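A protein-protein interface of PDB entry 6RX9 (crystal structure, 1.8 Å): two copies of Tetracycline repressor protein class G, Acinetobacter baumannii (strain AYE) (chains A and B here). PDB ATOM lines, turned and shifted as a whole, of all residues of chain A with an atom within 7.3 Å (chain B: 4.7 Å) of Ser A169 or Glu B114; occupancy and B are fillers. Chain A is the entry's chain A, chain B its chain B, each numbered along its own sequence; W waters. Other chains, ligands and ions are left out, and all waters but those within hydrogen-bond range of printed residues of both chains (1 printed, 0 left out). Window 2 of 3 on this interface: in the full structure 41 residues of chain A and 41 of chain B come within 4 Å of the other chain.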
ATOM      1  N   ALA A 167       1.828  15.095  19.855  1.00  0.00           N
ATOM      2  CA  ALA A 167       1.938  14.692  18.432  1.00  0.00           C
ATOM      3  C   ALA A 167       3.056  15.479  17.751  1.00  0.00           C
ATOM      4  O   ALA A 167       3.095  16.704  17.847  1.00  0.00           O
ATOM      5  CB  ALA A 167       0.619  14.906  17.728  1.00  0.00           C
ATOM      6  N   PRO A 168       3.997  14.808  17.043  1.00  0.00           N
ATOM      7  CA  PRO A 168       5.033  15.512  16.286  1.00  0.00           C
ATOM      8  C   PRO A 168       4.457  16.230  15.055  1.00  0.00           C
ATOM      9  O   PRO A 168       3.435  15.807  14.546  1.00  0.00           O
ATOM     10  CB  PRO A 168       6.019  14.405  15.882  1.00  0.00           C
ATOM     11  CG  PRO A 168       5.192  13.133  15.889  1.00  0.00           C
ATOM     12  CD  PRO A 168       4.126  13.345  16.945  1.00  0.00           C
ATOM     13  N   SER A 169       5.121  17.304  14.620  1.00  0.00           N
ATOM     14  CA  SER A 169       4.744  18.115  13.433  1.00  0.00           C
ATOM     15  C   SER A 169       4.909  17.278  12.158  1.00  0.00           C
ATOM     16  O   SER A 169       5.525  16.192  12.232  1.00  0.00           O
ATOM     17  CB  SER A 169       5.562  19.378  13.365  1.00  0.00           C
ATOM     18  OG  SER A 169       6.941  19.074  13.214  1.00  0.00           O
ATOM     19  N   SER A 170       4.393  17.780  11.032  1.00  0.00           N
ATOM     20  CA  SER A 170       4.487  17.146   9.690  1.00  0.00           C
ATOM     21  C   SER A 170       5.956  16.945   9.290  1.00  0.00           C
ATOM     22  O   SER A 170       6.226  15.993   8.536  1.00  0.00           O
ATOM     23  CB  SER A 170       3.750  17.955   8.658  1.00  0.00           C
ATOM     24  OG  SER A 170       4.225  19.292   8.634  1.00  0.00           O
ATOM     25  N   PHE A 171       6.865  17.806   9.766  1.00  0.00           N
ATOM     26  CA  PHE A 171       8.319  17.753   9.456  1.00  0.00           C
ATOM     27  C   PHE A 171       8.930  16.458  10.001  1.00  0.00           C
ATOM     28  O   PHE A 171       9.748  15.845   9.285  1.00  0.00           O
ATOM     29  CB  PHE A 171       9.062  18.963  10.034  1.00  0.00           C
ATOM     30  CG  PHE A 171      10.523  19.028   9.661  1.00  0.00           C
ATOM     31  CD1 PHE A 171      10.924  19.586   8.456  1.00  0.00           C
ATOM     32  CD2 PHE A 171      11.497  18.520  10.507  1.00  0.00           C
ATOM     33  CE1 PHE A 171      12.266  19.637   8.109  1.00  0.00           C
ATOM     34  CE2 PHE A 171      12.839  18.570  10.158  1.00  0.00           C
ATOM     35  CZ  PHE A 171      13.221  19.134   8.962  1.00  0.00           C
ATOM     36  N   LEU A 172       8.552  16.059  11.221  1.00  0.00           N
ATOM     37  CA  LEU A 172       9.215  14.958  11.974  1.00  0.00           C
ATOM     38  C   LEU A 172       8.416  13.649  11.893  1.00  0.00           C
ATOM     39  O   LEU A 172       9.038  12.591  12.113  1.00  0.00           O
ATOM     40  CB  LEU A 172       9.406  15.380  13.437  1.00  0.00           C
ATOM     41  CG  LEU A 172      10.646  16.223  13.743  1.00  0.00           C
ATOM     42  CD1 LEU A 172      10.906  16.268  15.241  1.00  0.00           C
ATOM     43  CD2 LEU A 172      11.878  15.698  13.018  1.00  0.00           C
ATOM     44  N   HIS A 173       7.112  13.700  11.597  1.00  0.00           N
ATOM     45  CA  HIS A 173       6.187  12.540  11.732  1.00  0.00           C
ATOM     46  C   HIS A 173       6.727  11.320  10.973  1.00  0.00           C
ATOM     47  O   HIS A 173       7.013  10.307  11.633  1.00  0.00           O
ATOM     48  CB  HIS A 173       4.763  12.888  11.277  1.00  0.00           C
ATOM     49  CG  HIS A 173       3.798  11.773  11.504  1.00  0.00           C
ATOM     50  ND1 HIS A 173       3.594  11.221  12.756  1.00  0.00           N
ATOM     51  CD2 HIS A 173       2.993  11.096  10.657  1.00  0.00           C
ATOM     52  CE1 HIS A 173       2.703  10.255  12.668  1.00  0.00           C
ATOM     53  NE2 HIS A 173       2.315  10.160  11.392  1.00  0.00           N
ATOM     54  N   ASP A 174       6.848  11.414   9.645  1.00  0.00           N
ATOM     55  CA  ASP A 174       7.191  10.268   8.756  1.00  0.00           C
ATOM     56  C   ASP A 174       8.655   9.860   8.965  1.00  0.00           C
ATOM     57  O   ASP A 174       8.920   8.638   8.997  1.00  0.00           O
ATOM     58  CB  ASP A 174       6.876  10.586   7.292  1.00  0.00           C
ATOM     59  CG  ASP A 174       5.392  10.564   6.964  1.00  0.00           C
ATOM     60  OD1 ASP A 174       4.588  10.276   7.875  1.00  0.00           O
ATOM     61  OD2 ASP A 174       5.048  10.835   5.798  1.00  0.00           O
ATOM     62  N   PHE A 176      10.411   9.957  11.731  1.00  0.00           N
ATOM     63  CA  PHE A 176      10.435   9.207  13.017  1.00  0.00           C
ATOM     64  C   PHE A 176       9.805   7.819  12.837  1.00  0.00           C
ATOM     65  O   PHE A 176      10.299   6.864  13.467  1.00  0.00           O
ATOM     66  CB  PHE A 176       9.748  10.016  14.122  1.00  0.00           C
ATOM     67  CG  PHE A 176      10.655  10.961  14.872  1.00  0.00           C
ATOM     68  CD1 PHE A 176      11.755  11.547  14.258  1.00  0.00           C
ATOM     69  CD2 PHE A 176      10.401  11.276  16.198  1.00  0.00           C
ATOM     70  CE1 PHE A 176      12.584  12.410  14.957  1.00  0.00           C
ATOM     71  CE2 PHE A 176      11.229  12.145  16.894  1.00  0.00           C
ATOM     72  CZ  PHE A 176      12.318  12.710  16.273  1.00  0.00           C
ATOM     73  N   PHE B 110       9.429  17.071  21.146  1.00  0.00           N
ATOM     74  CA  PHE B 110       9.449  17.162  19.660  1.00  0.00           C
ATOM     75  C   PHE B 110       9.871  18.569  19.216  1.00  0.00           C
ATOM     76  O   PHE B 110      10.479  18.686  18.132  1.00  0.00           O
ATOM     77  CB  PHE B 110       8.089  16.768  19.076  1.00  0.00           C
ATOM     78  CG  PHE B 110       7.681  15.340  19.336  1.00  0.00           C
ATOM     79  CD1 PHE B 110       8.514  14.287  18.985  1.00  0.00           C
ATOM     80  CD2 PHE B 110       6.459  15.044  19.922  1.00  0.00           C
ATOM     81  CE1 PHE B 110       8.137  12.973  19.222  1.00  0.00           C
ATOM     82  CE2 PHE B 110       6.083  13.729  20.156  1.00  0.00           C
ATOM     83  CZ  PHE B 110       6.923  12.697  19.807  1.00  0.00           C
ATOM     84  N   GLY B 111       9.548  19.596  20.010  1.00  0.00           N
ATOM     85  CA  GLY B 111       9.993  20.985  19.784  1.00  0.00           C
ATOM     86  C   GLY B 111      11.509  21.081  19.760  1.00  0.00           C
ATOM     87  O   GLY B 111      12.060  21.610  18.774  1.00  0.00           O
ATOM     88  N   THR B 112      12.159  20.565  20.808  1.00  0.00           N
ATOM     89  CA  THR B 112      13.637  20.528  20.973  1.00  0.00           C
ATOM     90  C   THR B 112      14.253  19.687  19.848  1.00  0.00           C
ATOM     91  O   THR B 112      15.194  20.183  19.194  1.00  0.00           O
ATOM     92  CB  THR B 112      14.014  20.006  22.364  1.00  0.00           C
ATOM     93  OG1 THR B 112      13.512  20.950  23.310  1.00  0.00           O
ATOM     94  CG2 THR B 112      15.506  19.832  22.558  1.00  0.00           C
ATOM     95  N   ALA B 113      13.734  18.474  19.631  1.00  0.00           N
ATOM     96  CA  ALA B 113      14.221  17.509  18.614  1.00  0.00           C
ATOM     97  C   ALA B 113      14.197  18.159  17.224  1.00  0.00           C
ATOM     98  O   ALA B 113      15.217  18.063  16.514  1.00  0.00           O
ATOM     99  CB  ALA B 113      13.392  16.250  18.645  1.00  0.00           C
ATOM    100  N   GLU B 114      13.084  18.804  16.855  1.00  0.00           N
ATOM    101  CA  GLU B 114      12.909  19.438  15.520  1.00  0.00           C
ATOM    102  C   GLU B 114      13.979  20.520  15.323  1.00  0.00           C
ATOM    103  O   GLU B 114      14.599  20.536  14.244  1.00  0.00           O
ATOM    104  CB  GLU B 114      11.499  20.011  15.345  1.00  0.00           C
ATOM    105  CG  GLU B 114      11.322  20.757  14.031  1.00  0.00           C
ATOM    106  CD  GLU B 114       9.901  20.890  13.508  1.00  0.00           C
ATOM    107  OE1 GLU B 114       8.980  20.331  14.132  1.00  0.00           O
ATOM    108  OE2 GLU B 114       9.722  21.558  12.470  1.00  0.00           O
ATOM    109  N   THR B 115      14.191  21.383  16.323  1.00  0.00           N
ATOM    110  CA  THR B 115      15.193  22.483  16.284  1.00  0.00           C
ATOM    111  C   THR B 115      16.590  21.887  16.060  1.00  0.00           C
ATOM    112  O   THR B 115      17.309  22.380  15.169  1.00  0.00           O
ATOM    113  CB  THR B 115      15.121  23.352  17.546  1.00  0.00           C
ATOM    114  OG1 THR B 115      13.828  23.954  17.579  1.00  0.00           O
ATOM    115  CG2 THR B 115      16.180  24.431  17.587  1.00  0.00           C
ATOM    116  N   GLN B 116      16.946  20.853  16.826  1.00  0.00           N
ATOM    117  CA  GLN B 116      18.258  20.158  16.739  1.00  0.00           C
ATOM    118  C   GLN B 116      18.434  19.543  15.343  1.00  0.00           C
ATOM    119  O   GLN B 116      19.521  19.711  14.760  1.00  0.00           O
ATOM    120  CB  GLN B 116      18.357  19.064  17.802  1.00  0.00           C
ATOM    121  CG  GLN B 116      18.429  19.587  19.229  1.00  0.00           C
ATOM    122  CD  GLN B 116      18.438  18.456  20.229  1.00  0.00           C
ATOM    123  OE1 GLN B 116      18.030  17.337  19.928  1.00  0.00           O
ATOM    124  NE2 GLN B 116      18.912  18.736  21.432  1.00  0.00           N
ATOM    125  N   ILE B 117      17.413  18.836  14.847  1.00  0.00           N
ATOM    126  CA  ILE B 117      17.458  18.077  13.560  1.00  0.00           C
ATOM    127  C   ILE B 117      17.509  19.071  12.390  1.00  0.00           C
ATOM    128  O   ILE B 117      18.342  18.863  11.488  1.00  0.00           O
ATOM    129  CB  ILE B 117      16.276  17.091  13.456  1.00  0.00           C
ATOM    130  CG1 ILE B 117      16.411  15.952  14.471  1.00  0.00           C
ATOM    131  CG2 ILE B 117      16.126  16.556  12.038  1.00  0.00           C
ATOM    132  CD1 ILE B 117      15.112  15.240  14.780  1.00  0.00           C
ATOM    133  N   ARG B 118      16.664  20.107  12.402  1.00  0.00           N
ATOM    134  CA  ARG B 118      16.675  21.187  11.373  1.00  0.00           C
ATOM    135  C   ARG B 118      18.089  21.774  11.276  1.00  0.00           C
ATOM    136  O   ARG B 118      18.600  21.903  10.146  1.00  0.00           O
ATOM    137  CB  ARG B 118      15.653  22.283  11.693  1.00  0.00           C
ATOM    138  CG  ARG B 118      14.236  21.969  11.237  1.00  0.00           C
ATOM    139  CD  ARG B 118      13.297  23.142  11.458  1.00  0.00           C
ATOM    140  NE  ARG B 118      11.913  22.833  11.120  1.00  0.00           N
ATOM    141  CZ  ARG B 118      11.402  22.826   9.889  1.00  0.00           C
ATOM    142  NH1 ARG B 118      10.125  22.532   9.710  1.00  0.00           N
ATOM    143  NH2 ARG B 118      12.159  23.106   8.841  1.00  0.00           N
HETATM  144  O   HOH W   1       7.086  21.956  12.222  1.00  0.00           O
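The side-chain carboxylate (OE1) of Glu B114 sits at hydrogen-bond distance from the side-chain hydroxyl (OG) of Ser A169 (2.6 Å).
The guanidinium group of Arg B118 lies within salt-bridge range of the side-chain carboxylate of Glu B114 (2.9 Å).
Phe B110 touches Pro A168 (CE2 to CD, 3.8 Å). Phe A171 touches Glu B114 (CB to OE2, 3.6 Å). Phe A171 touches Arg B118. Leu A172 touches Phe B110. Glu B114 touches Leu A172. Leu A172 touches Ile B117. Phe B110 touches Phe A176 (CE1 to CE2, 3.96 Å). Phe A176 touches Ile B117.
Of chain B, only Glu B114 comes within 4 Å of Ser A169. Of chain A, only Ser A169, Phe A171 and Leu A172 come within 4 Å of Glu B114. No residue of chain A comes within 4 Å of Ala B113. Of the printed residues of chain B, Pro A168 touches Phe B110 (3.8 Å). Printed residues of chain B within 4 Å of Phe A171: Glu B114 (3.6 Å) and Arg B118 (3.3 Å). Printed residues of chain A within 4 Å of Ile B117: Leu A172 (3.7 Å) and Phe A176 (3.8 Å). Of the printed residues of chain B, Leu A172 touches Phe B110 (3.8 Å), Glu B114 (3.7 Å) and Ile B117 (3.7 Å). Printed residues of chain A within 4 Å of Arg B118: Phe A171 (3.3 Å). The nearest printed residue of chain B that does not touch Ser A169 is Phe B110 (5.4 Å). The nearest printed residue of chain A that does not touch Arg B118 is Ser A169 (5.9 Å).
Of the 9 printed residues of chain B, 4 touch a printed residue of chain A. Printed residues of chain B that touch a printed residue of chain A: Phe B110, Glu B114, Ile B117 and Arg B118. Hydrophobic or aromatic side chains of chain B that line the printed part of chain A: Phe B110 and Ile B117. Printed residues of chain A that touch a printed residue of chain B: Pro A168, Ser A169, Phe A171, Leu A172 and Phe A176. Among the printed residues, no Asp or Glu carboxylate lies within 4 Å of a Lys or Arg side-chain nitrogen of the other chain.
No position is printed for both chains.
Water W1 lies within hydrogen-bond range of OE2 of Glu B114 (2.7 Å) and OG of Ser A169 (3.1 Å).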
